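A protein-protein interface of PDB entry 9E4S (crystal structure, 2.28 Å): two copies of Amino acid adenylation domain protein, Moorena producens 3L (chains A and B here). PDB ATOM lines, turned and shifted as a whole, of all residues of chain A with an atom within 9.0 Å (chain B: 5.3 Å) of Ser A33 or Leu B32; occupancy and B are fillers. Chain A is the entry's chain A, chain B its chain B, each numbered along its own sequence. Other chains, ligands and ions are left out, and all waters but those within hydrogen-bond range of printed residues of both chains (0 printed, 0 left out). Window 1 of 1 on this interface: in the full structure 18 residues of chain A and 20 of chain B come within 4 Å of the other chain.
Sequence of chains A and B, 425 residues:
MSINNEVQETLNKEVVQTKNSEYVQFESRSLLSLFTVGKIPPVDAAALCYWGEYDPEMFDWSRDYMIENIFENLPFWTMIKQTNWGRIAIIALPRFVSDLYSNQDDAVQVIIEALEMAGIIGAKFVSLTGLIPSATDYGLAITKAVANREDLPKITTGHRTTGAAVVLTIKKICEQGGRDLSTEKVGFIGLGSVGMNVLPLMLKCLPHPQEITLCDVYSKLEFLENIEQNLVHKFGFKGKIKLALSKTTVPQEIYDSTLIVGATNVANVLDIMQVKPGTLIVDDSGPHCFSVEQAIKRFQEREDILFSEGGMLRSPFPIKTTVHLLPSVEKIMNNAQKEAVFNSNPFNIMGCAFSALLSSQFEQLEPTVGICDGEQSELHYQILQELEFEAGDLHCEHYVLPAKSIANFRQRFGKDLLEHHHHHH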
ATOM      1  N   GLU A  27      -9.269  28.252  20.125  1.00  0.00           N
ATOM      2  CA  GLU A  27      -9.714  27.461  21.264  1.00  0.00           C
ATOM      3  C   GLU A  27      -8.698  26.356  21.500  1.00  0.00           C
ATOM      4  O   GLU A  27      -8.461  25.526  20.616  1.00  0.00           O
ATOM      5  CB  GLU A  27     -11.109  26.874  21.027  1.00  0.00           C
ATOM      6  CG  GLU A  27     -12.185  27.391  21.979  1.00  0.00           C
ATOM      7  CD  GLU A  27     -11.961  26.981  23.428  1.00  0.00           C
ATOM      8  OE1 GLU A  27     -11.101  26.111  23.689  1.00  0.00           O
ATOM      9  OE2 GLU A  27     -12.655  27.529  24.311  1.00  0.00           O
ATOM     10  N   ARG A  29      -8.988  23.932  23.633  1.00  0.00           N
ATOM     11  CA  ARG A  29      -9.650  22.685  23.978  1.00  0.00           C
ATOM     12  C   ARG A  29     -10.367  22.092  22.767  1.00  0.00           C
ATOM     13  O   ARG A  29     -10.681  22.783  21.795  1.00  0.00           O
ATOM     14  CB  ARG A  29     -10.636  22.906  25.126  1.00  0.00           C
ATOM     15  CG  ARG A  29      -9.989  23.499  26.368  1.00  0.00           C
ATOM     16  CD  ARG A  29     -10.954  23.536  27.534  1.00  0.00           C
ATOM     17  NE  ARG A  29     -11.993  24.541  27.359  1.00  0.00           N
ATOM     18  CZ  ARG A  29     -12.978  24.748  28.222  1.00  0.00           C
ATOM     19  NH1 ARG A  29     -13.089  24.031  29.330  1.00  0.00           N
ATOM     20  NH2 ARG A  29     -13.877  25.696  27.968  1.00  0.00           N
ATOM     21  N   SER A  30     -10.621  20.786  22.846  1.00  0.00           N
ATOM     22  CA  SER A  30     -11.218  20.048  21.739  1.00  0.00           C
ATOM     23  C   SER A  30     -12.616  20.566  21.423  1.00  0.00           C
ATOM     24  O   SER A  30     -13.460  20.697  22.314  1.00  0.00           O
ATOM     25  CB  SER A  30     -11.271  18.557  22.084  1.00  0.00           C
ATOM     26  OG  SER A  30     -12.368  17.919  21.450  1.00  0.00           O
ATOM     27  N   LEU A  31     -12.865  20.854  20.143  1.00  0.00           N
ATOM     28  CA  LEU A  31     -14.195  21.307  19.745  1.00  0.00           C
ATOM     29  C   LEU A  31     -15.235  20.213  19.940  1.00  0.00           C
ATOM     30  O   LEU A  31     -16.386  20.499  20.295  1.00  0.00           O
ATOM     31  CB  LEU A  31     -14.179  21.778  18.294  1.00  0.00           C
ATOM     32  CG  LEU A  31     -13.297  22.981  17.983  1.00  0.00           C
ATOM     33  CD1 LEU A  31     -13.491  23.398  16.539  1.00  0.00           C
ATOM     34  CD2 LEU A  31     -13.611  24.141  18.921  1.00  0.00           C
ATOM     35  N   LEU A  32     -14.852  18.956  19.707  1.00  0.00           N
ATOM     36  CA  LEU A  32     -15.784  17.855  19.916  1.00  0.00           C
ATOM     37  C   LEU A  32     -16.168  17.736  21.385  1.00  0.00           C
ATOM     38  O   LEU A  32     -17.353  17.600  21.711  1.00  0.00           O
ATOM     39  CB  LEU A  32     -15.177  16.548  19.403  1.00  0.00           C
ATOM     40  CG  LEU A  32     -16.087  15.321  19.455  1.00  0.00           C
ATOM     41  CD1 LEU A  32     -17.325  15.547  18.599  1.00  0.00           C
ATOM     42  CD2 LEU A  32     -15.339  14.074  18.997  1.00  0.00           C
ATOM     43  N   SER A  33     -15.183  17.795  22.286  1.00  0.00           N
ATOM     44  CA  SER A  33     -15.482  17.712  23.713  1.00  0.00           C
ATOM     45  C   SER A  33     -16.340  18.885  24.167  1.00  0.00           C
ATOM     46  O   SER A  33     -17.311  18.704  24.913  1.00  0.00           O
ATOM     47  CB  SER A  33     -14.186  17.656  24.521  1.00  0.00           C
ATOM     48  OG  SER A  33     -13.422  16.514  24.175  1.00  0.00           O
ATOM     49  N   LEU A  34     -16.001  20.098  23.725  1.00  0.00           N
ATOM     50  CA  LEU A  34     -16.788  21.263  24.115  1.00  0.00           C
ATOM     51  C   LEU A  34     -18.216  21.168  23.596  1.00  0.00           C
ATOM     52  O   LEU A  34     -19.144  21.672  24.237  1.00  0.00           O
ATOM     53  CB  LEU A  34     -16.118  22.542  23.615  1.00  0.00           C
ATOM     54  CG  LEU A  34     -14.830  22.921  24.346  1.00  0.00           C
ATOM     55  CD1 LEU A  34     -14.008  23.868  23.501  1.00  0.00           C
ATOM     56  CD2 LEU A  34     -15.150  23.547  25.694  1.00  0.00           C
ATOM     57  N   PHE A  35     -18.415  20.516  22.450  1.00  0.00           N
ATOM     58  CA  PHE A  35     -19.769  20.325  21.945  1.00  0.00           C
ATOM     59  C   PHE A  35     -20.553  19.357  22.825  1.00  0.00           C
ATOM     60  O   PHE A  35     -21.728  19.599  23.123  1.00  0.00           O
ATOM     61  CB  PHE A  35     -19.728  19.831  20.497  1.00  0.00           C
ATOM     62  CG  PHE A  35     -21.027  19.244  20.015  1.00  0.00           C
ATOM     63  CD1 PHE A  35     -22.067  20.064  19.604  1.00  0.00           C
ATOM     64  CD2 PHE A  35     -21.209  17.869  19.973  1.00  0.00           C
ATOM     65  CE1 PHE A  35     -23.261  19.524  19.161  1.00  0.00           C
ATOM     66  CE2 PHE A  35     -22.399  17.325  19.532  1.00  0.00           C
ATOM     67  CZ  PHE A  35     -23.426  18.152  19.125  1.00  0.00           C
ATOM     68  N   THR A  36     -19.921  18.263  23.263  1.00  0.00           N
ATOM     69  CA  THR A  36     -20.661  17.254  24.015  1.00  0.00           C
ATOM     70  C   THR A  36     -21.068  17.742  25.401  1.00  0.00           C
ATOM     71  O   THR A  36     -21.970  17.155  26.007  1.00  0.00           O
ATOM     72  CB  THR A  36     -19.848  15.958  24.132  1.00  0.00           C
ATOM     73  OG1 THR A  36     -18.601  16.212  24.789  1.00  0.00           O
ATOM     74  CG2 THR A  36     -19.573  15.381  22.751  1.00  0.00           C
ATOM     75  N   VAL A  37     -20.441  18.802  25.912  1.00  0.00           N
ATOM     76  CA  VAL A  37     -20.822  19.379  27.196  1.00  0.00           C
ATOM     77  C   VAL A  37     -21.729  20.595  27.028  1.00  0.00           C
ATOM     78  O   VAL A  37     -21.949  21.336  27.990  1.00  0.00           O
ATOM     79  CB  VAL A  37     -19.585  19.738  28.032  1.00  0.00           C
ATOM     80  CG1 VAL A  37     -18.778  18.493  28.334  1.00  0.00           C
ATOM     81  CG2 VAL A  37     -18.740  20.766  27.301  1.00  0.00           C
ATOM     82  N   GLY A  38     -22.253  20.821  25.826  1.00  0.00           N
ATOM     83  CA  GLY A  38     -23.188  21.904  25.591  1.00  0.00           C
ATOM     84  C   GLY A  38     -22.593  23.294  25.540  1.00  0.00           C
ATOM     85  O   GLY A  38     -23.342  24.272  25.650  1.00  0.00           O
ATOM     86  N   LYS A  39     -21.277  23.422  25.374  1.00  0.00           N
ATOM     87  CA  LYS A  39     -20.634  24.725  25.266  1.00  0.00           C
ATOM     88  C   LYS A  39     -20.533  25.229  23.832  1.00  0.00           C
ATOM     89  O   LYS A  39     -20.263  26.418  23.629  1.00  0.00           O
ATOM     90  CB  LYS A  39     -19.232  24.680  25.883  1.00  0.00           C
ATOM     91  CG  LYS A  39     -19.207  24.765  27.401  1.00  0.00           C
ATOM     92  CD  LYS A  39     -17.779  24.755  27.931  1.00  0.00           C
ATOM     93  CE  LYS A  39     -17.749  24.817  29.447  1.00  0.00           C
ATOM     94  NZ  LYS A  39     -18.258  26.121  29.949  1.00  0.00           N
ATOM     95  N   ILE A  40     -20.741  24.365  22.836  1.00  0.00           N
ATOM     96  CA  ILE A  40     -20.679  24.744  21.436  1.00  0.00           C
ATOM     97  C   ILE A  40     -21.976  24.302  20.758  1.00  0.00           C
ATOM     98  O   ILE A  40     -22.297  23.109  20.782  1.00  0.00           O
ATOM     99  CB  ILE A  40     -19.470  24.135  20.710  1.00  0.00           C
ATOM    100  CG1 ILE A  40     -18.178  24.811  21.168  1.00  0.00           C
ATOM    101  CG2 ILE A  40     -19.631  24.256  19.200  1.00  0.00           C
ATOM    102  CD1 ILE A  40     -16.952  24.303  20.457  1.00  0.00           C
ATOM    103  N   LEU A  74      -8.181   9.288  12.800  1.00  0.00           N
ATOM    104  CA  LEU A  74      -9.499   9.776  13.160  1.00  0.00           C
ATOM    105  C   LEU A  74      -9.718  11.166  12.590  1.00  0.00           C
ATOM    106  O   LEU A  74      -8.770  11.949  12.472  1.00  0.00           O
ATOM    107  CB  LEU A  74      -9.675   9.814  14.684  1.00  0.00           C
ATOM    108  CG  LEU A  74      -9.735   8.451  15.374  1.00  0.00           C
ATOM    109  CD1 LEU A  74      -9.647   8.620  16.880  1.00  0.00           C
ATOM    110  CD2 LEU A  74     -11.005   7.715  14.983  1.00  0.00           C
ATOM    111  N   PRO A  75     -10.955  11.496  12.219  1.00  0.00           N
ATOM    112  CA  PRO A  75     -11.236  12.852  11.739  1.00  0.00           C
ATOM    113  C   PRO A  75     -11.032  13.865  12.853  1.00  0.00           C
ATOM    114  O   PRO A  75     -11.219  13.566  14.035  1.00  0.00           O
ATOM    115  CB  PRO A  75     -12.705  12.783  11.303  1.00  0.00           C
ATOM    116  CG  PRO A  75     -13.015  11.316  11.179  1.00  0.00           C
ATOM    117  CD  PRO A  75     -12.148  10.637  12.186  1.00  0.00           C
ATOM    118  N   TRP A  77     -12.140  17.602  13.939  1.00  0.00           N
ATOM    119  CA  TRP A  77     -12.941  18.823  13.867  1.00  0.00           C
ATOM    120  C   TRP A  77     -12.059  19.996  14.276  1.00  0.00           C
ATOM    121  O   TRP A  77     -11.787  20.200  15.460  1.00  0.00           O
ATOM    122  CB  TRP A  77     -14.164  18.701  14.769  1.00  0.00           C
ATOM    123  CG  TRP A  77     -15.097  19.872  14.703  1.00  0.00           C
ATOM    124  CD1 TRP A  77     -15.047  20.918  13.826  1.00  0.00           C
ATOM    125  CD2 TRP A  77     -16.227  20.115  15.550  1.00  0.00           C
ATOM    126  NE1 TRP A  77     -16.072  21.796  14.075  1.00  0.00           N
ATOM    127  CE2 TRP A  77     -16.813  21.326  15.128  1.00  0.00           C
ATOM    128  CE3 TRP A  77     -16.799  19.426  16.622  1.00  0.00           C
ATOM    129  CZ2 TRP A  77     -17.942  21.864  15.743  1.00  0.00           C
ATOM    130  CZ3 TRP A  77     -17.919  19.962  17.232  1.00  0.00           C
ATOM    131  CH2 TRP A  77     -18.478  21.170  16.792  1.00  0.00           C
ATOM    132  N   MET A 117     -19.283  11.504  12.173  1.00  0.00           N
ATOM    133  CA  MET A 117     -19.021  12.560  13.144  1.00  0.00           C
ATOM    134  C   MET A 117     -19.766  13.836  12.781  1.00  0.00           C
ATOM    135  O   MET A 117     -20.311  14.514  13.659  1.00  0.00           O
ATOM    136  CB  MET A 117     -17.520  12.830  13.239  1.00  0.00           C
ATOM    137  CG  MET A 117     -17.183  14.198  13.810  1.00  0.00           C
ATOM    138  SD  MET A 117     -15.415  14.541  13.809  1.00  0.00           S
ATOM    139  CE  MET A 117     -14.898  13.658  15.278  1.00  0.00           C
ATOM    140  N   ILE A 120     -23.336  13.743  13.941  1.00  0.00           N
ATOM    141  CA  ILE A 120     -23.536  13.843  15.383  1.00  0.00           C
ATOM    142  C   ILE A 120     -23.523  15.299  15.832  1.00  0.00           C
ATOM    143  O   ILE A 120     -24.289  15.694  16.720  1.00  0.00           O
ATOM    144  CB  ILE A 120     -22.476  13.007  16.127  1.00  0.00           C
ATOM    145  CG1 ILE A 120     -22.769  11.517  15.959  1.00  0.00           C
ATOM    146  CG2 ILE A 120     -22.404  13.395  17.600  1.00  0.00           C
ATOM    147  CD1 ILE A 120     -22.000  10.641  16.909  1.00  0.00           C
ATOM    148  N   ILE A 121     -22.666  16.120  15.225  1.00  0.00           N
ATOM    149  CA  ILE A 121     -22.541  17.519  15.621  1.00  0.00           C
ATOM    150  C   ILE A 121     -23.575  18.361  14.882  1.00  0.00           C
ATOM    151  O   ILE A 121     -23.566  19.594  14.973  1.00  0.00           O
ATOM    152  CB  ILE A 121     -21.114  18.044  15.381  1.00  0.00           C
ATOM    153  CG1 ILE A 121     -20.738  17.942  13.903  1.00  0.00           C
ATOM    154  CG2 ILE A 121     -20.114  17.279  16.236  1.00  0.00           C
ATOM    155  CD1 ILE A 121     -19.369  18.501  13.586  1.00  0.00           C
ATOM    156  N   HIS A 324      -9.372  25.524  16.181  1.00  0.00           N
ATOM    157  CA  HIS A 324      -8.751  24.642  17.160  1.00  0.00           C
ATOM    158  C   HIS A 324      -7.646  23.872  16.451  1.00  0.00           C
ATOM    159  O   HIS A 324      -7.922  23.047  15.575  1.00  0.00           O
ATOM    160  CB  HIS A 324      -9.779  23.696  17.777  1.00  0.00           C
ATOM    161  CG  HIS A 324      -9.178  22.633  18.639  1.00  0.00           C
ATOM    162  ND1 HIS A 324      -8.429  22.919  19.759  1.00  0.00           N
ATOM    163  CD2 HIS A 324      -9.217  21.282  18.546  1.00  0.00           C
ATOM    164  CE1 HIS A 324      -8.028  21.791  20.317  1.00  0.00           C
ATOM    165  NE2 HIS A 324      -8.494  20.783  19.602  1.00  0.00           N
ATOM    166  N   SER B  30      -8.971   8.336  21.807  1.00  0.00           N
ATOM    167  CA  SER B  30     -10.070   8.848  22.613  1.00  0.00           C
ATOM    168  C   SER B  30     -11.327   8.018  22.402  1.00  0.00           C
ATOM    169  O   SER B  30     -11.720   7.737  21.267  1.00  0.00           O
ATOM    170  CB  SER B  30     -10.353  10.306  22.263  1.00  0.00           C
ATOM    171  OG  SER B  30     -11.709  10.622  22.531  1.00  0.00           O
ATOM    172  N   LEU B  31     -11.965   7.636  23.509  1.00  0.00           N
ATOM    173  CA  LEU B  31     -13.219   6.900  23.416  1.00  0.00           C
ATOM    174  C   LEU B  31     -14.335   7.768  22.851  1.00  0.00           C
ATOM    175  O   LEU B  31     -15.213   7.262  22.141  1.00  0.00           O
ATOM    176  CB  LEU B  31     -13.609   6.359  24.792  1.00  0.00           C
ATOM    177  CG  LEU B  31     -12.635   5.402  25.483  1.00  0.00           C
ATOM    178  CD1 LEU B  31     -13.245   4.902  26.778  1.00  0.00           C
ATOM    179  CD2 LEU B  31     -12.262   4.232  24.582  1.00  0.00           C
ATOM    180  N   LEU B  32     -14.323   9.069  23.152  1.00  0.00           N
ATOM    181  CA  LEU B  32     -15.337   9.965  22.603  1.00  0.00           C
ATOM    182  C   LEU B  32     -15.232  10.056  21.086  1.00  0.00           C
ATOM    183  O   LEU B  32     -16.247   9.986  20.383  1.00  0.00           O
ATOM    184  CB  LEU B  32     -15.210  11.351  23.238  1.00  0.00           C
ATOM    185  CG  LEU B  32     -16.215  12.419  22.795  1.00  0.00           C
ATOM    186  CD1 LEU B  32     -17.643  11.999  23.109  1.00  0.00           C
ATOM    187  CD2 LEU B  32     -15.891  13.755  23.453  1.00  0.00           C
ATOM    188  N   SER B  33     -14.012  10.213  20.563  1.00  0.00           N
ATOM    189  CA  SER B  33     -13.832  10.257  19.114  1.00  0.00           C
ATOM    190  C   SER B  33     -14.244   8.942  18.464  1.00  0.00           C
ATOM    191  O   SER B  33     -14.953   8.939  17.451  1.00  0.00           O
ATOM    192  CB  SER B  33     -12.379  10.588  18.771  1.00  0.00           C
ATOM    193  OG  SER B  33     -12.022  11.874  19.249  1.00  0.00           O
ATOM    194  N   LEU B  34     -13.814   7.814  19.035  1.00  0.00           N
ATOM    195  CA  LEU B  34     -14.177   6.520  18.466  1.00  0.00           C
ATOM    196  C   LEU B  34     -15.685   6.311  18.474  1.00  0.00           C
ATOM    197  O   LEU B  34     -16.233   5.708  17.543  1.00  0.00           O
ATOM    198  CB  LEU B  34     -13.470   5.395  19.224  1.00  0.00           C
ATOM    199  CG  LEU B  34     -11.954   5.308  19.007  1.00  0.00           C
ATOM    200  CD1 LEU B  34     -11.294   4.485  20.102  1.00  0.00           C
ATOM    201  CD2 LEU B  34     -11.622   4.734  17.632  1.00  0.00           C
ATOM    202  N   PHE B  35     -16.377   6.818  19.497  1.00  0.00           N
ATOM    203  CA  PHE B  35     -17.833   6.723  19.513  1.00  0.00           C
ATOM    204  C   PHE B  35     -18.451   7.513  18.364  1.00  0.00           C
ATOM    205  O   PHE B  35     -19.353   7.019  17.678  1.00  0.00           O
ATOM    206  CB  PHE B  35     -18.383   7.214  20.854  1.00  0.00           C
ATOM    207  CG  PHE B  35     -19.854   7.517  20.825  1.00  0.00           C
ATOM    208  CD1 PHE B  35     -20.787   6.498  20.943  1.00  0.00           C
ATOM    209  CD2 PHE B  35     -20.305   8.817  20.658  1.00  0.00           C
ATOM    210  CE1 PHE B  35     -22.140   6.772  20.912  1.00  0.00           C
ATOM    211  CE2 PHE B  35     -21.656   9.097  20.619  1.00  0.00           C
ATOM    212  CZ  PHE B  35     -22.575   8.073  20.747  1.00  0.00           C
ATOM    213  N   THR B  36     -17.979   8.742  18.137  1.00  0.00           N
ATOM    214  CA  THR B  36     -18.607   9.593  17.136  1.00  0.00           C
ATOM    215  C   THR B  36     -18.396   9.079  15.714  1.00  0.00           C
ATOM    216  O   THR B  36     -19.176   9.439  14.822  1.00  0.00           O
ATOM    217  CB  THR B  36     -18.101  11.040  17.261  1.00  0.00           C
ATOM    218  OG1 THR B  36     -16.671  11.080  17.143  1.00  0.00           O
ATOM    219  CG2 THR B  36     -18.512  11.638  18.602  1.00  0.00           C
ATOM    220  N   LEU B  74     -12.773  19.700  31.645  1.00  0.00           N
ATOM    221  CA  LEU B  74     -13.681  18.928  30.814  1.00  0.00           C
ATOM    222  C   LEU B  74     -13.828  17.520  31.364  1.00  0.00           C
ATOM    223  O   LEU B  74     -12.878  16.964  31.924  1.00  0.00           O
ATOM    224  CB  LEU B  74     -13.181  18.850  29.365  1.00  0.00           C
ATOM    225  CG  LEU B  74     -13.302  20.119  28.528  1.00  0.00           C
ATOM    226  CD1 LEU B  74     -12.403  20.017  27.308  1.00  0.00           C
ATOM    227  CD2 LEU B  74     -14.748  20.346  28.127  1.00  0.00           C
ATOM    228  N   TRP B  77     -14.058  10.750  29.412  1.00  0.00           N
ATOM    229  CA  TRP B  77     -14.574   9.388  29.264  1.00  0.00           C
ATOM    230  C   TRP B  77     -13.393   8.428  29.227  1.00  0.00           C
ATOM    231  O   TRP B  77     -12.686   8.331  28.221  1.00  0.00           O
ATOM    232  CB  TRP B  77     -15.421   9.282  28.000  1.00  0.00           C
ATOM    233  CG  TRP B  77     -16.052   7.933  27.784  1.00  0.00           C
ATOM    234  CD1 TRP B  77     -16.071   6.883  28.656  1.00  0.00           C
ATOM    235  CD2 TRP B  77     -16.758   7.493  26.614  1.00  0.00           C
ATOM    236  NE1 TRP B  77     -16.740   5.819  28.103  1.00  0.00           N
ATOM    237  CE2 TRP B  77     -17.174   6.167  26.851  1.00  0.00           C
ATOM    238  CE3 TRP B  77     -17.077   8.092  25.392  1.00  0.00           C
ATOM    239  CZ2 TRP B  77     -17.891   5.429  25.910  1.00  0.00           C
ATOM    240  CZ3 TRP B  77     -17.791   7.357  24.460  1.00  0.00           C
ATOM    241  CH2 TRP B  77     -18.189   6.039  24.725  1.00  0.00           C
ATOM    242  N   MET B 117     -22.489  15.169  28.384  1.00  0.00           N
ATOM    243  CA  MET B 117     -21.682  14.226  27.617  1.00  0.00           C
ATOM    244  C   MET B 117     -22.201  12.801  27.773  1.00  0.00           C
ATOM    245  O   MET B 117     -22.213  12.031  26.808  1.00  0.00           O
ATOM    246  CB  MET B 117     -20.221  14.311  28.051  1.00  0.00           C
ATOM    247  CG  MET B 117     -19.320  13.311  27.354  1.00  0.00           C
ATOM    248  SD  MET B 117     -17.703  13.177  28.133  1.00  0.00           S
ATOM    249  CE  MET B 117     -16.737  14.240  27.064  1.00  0.00           C
ATOM    250  N   ILE B 121     -23.584   9.974  24.645  1.00  0.00           N
ATOM    251  CA  ILE B 121     -23.080   8.640  24.338  1.00  0.00           C
ATOM    252  C   ILE B 121     -24.119   7.584  24.701  1.00  0.00           C
ATOM    253  O   ILE B 121     -23.840   6.381  24.650  1.00  0.00           O
ATOM    254  CB  ILE B 121     -21.740   8.374  25.045  1.00  0.00           C
ATOM    255  CG1 ILE B 121     -21.890   8.508  26.559  1.00  0.00           C
ATOM    256  CG2 ILE B 121     -20.671   9.328  24.527  1.00  0.00           C
ATOM    257  CD1 ILE B 121     -20.616   8.198  27.315  1.00  0.00           C
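O of Thr A36 sits at hydrogen-bond distance from N of Met B117, 3.1 Å away.
The backbone NH (N) of Met A117 is in hydrogen-bond range of the backbone carbonyl oxygen (O) of Thr B36, 3.4 Å away.
OG1 of Thr B36 sits at hydrogen-bond distance from O of Ser B33 (2.8 Å).
The backbone NH (N) of Ser B33 sits at hydrogen-bond distance from the side-chain hydroxyl (OG) of Ser B30 (3.1 Å).
OG1 of Thr A36 is in hydrogen-bond range of O of Ser A33 (2.8 Å).
OE1 of Glu A27 is in hydrogen-bond range of N of Arg A29.
The backbone NH (N) of Leu B32 lies within hydrogen-bond range of the side-chain hydroxyl (OG) of Ser B30 (3.1 Å).
N of Leu A32 is in hydrogen-bond range of OG of Ser A30 (3.2 Å).
Among the printed residues, merely in contact across the chains: Arg A29 with Leu B74 (3.8 Å), Leu A32 with Ser B33 (3.99 Å), Leu A32 with Thr B36 (3.8 Å), Ser A33 with Leu B32 (3.8 Å), Thr A36 with Leu B32 (3.9 Å), Leu A74 with Ser B33 (3.9 Å) and Ile A120 with Thr B36 (3.6 Å).
Printed residues of chain B within 4 Å of Arg A29: Leu B74.
Of the printed residues of chain B, Ser A33 touches Leu B32.
Of the printed residues of chain B, Thr A36 touches Leu B32 and Met B117.
Printed residues of chain B within 4 Å of Ile A120: Thr B36 (3.6 Å).
Of the printed residues of chain A, Thr B36 touches Leu A32, Met A117 and Ile A120.
Printed residues of chain A within 4 Å of Leu B74: Arg A29.
Hydrophobic or aromatic side chains of chain B within 4 Å of the printed part of chain A: Leu B32, Leu B74 and Met B117.
Of the 20 printed residues of chain A, 7 touch a printed residue of chain B.
Hydrophobic or aromatic side chains of chain A that line the printed part of chain B: Leu A32, Leu A74, Met A117 and Ile A120.
Among the printed residues, no Asp or Glu carboxylate lies within 4 Å of a Lys or Arg side-chain nitrogen of the other chain.
Leu A32 touches Ser B33, and with the chains exchanged Ser A33 touches Leu B32.
Leu A32 touches Thr B36, and with the chains exchanged Thr A36 touches Leu B32.
Thr A36 touches Met B117, and with the chains exchanged Met A117 touches Thr B36.
Leu A74 touches Ser B33, but with the chains exchanged Ser A33 does not touch Leu B74 (4.1 Å).
Positions printed for both chains: 30, 31, 32, 33, 34, 35, 36, 74, 77, 117 and 121.
Of the 9 pairs that touch across the chains among the printed residues, 6 have their exchanged pair printed and touching as well.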
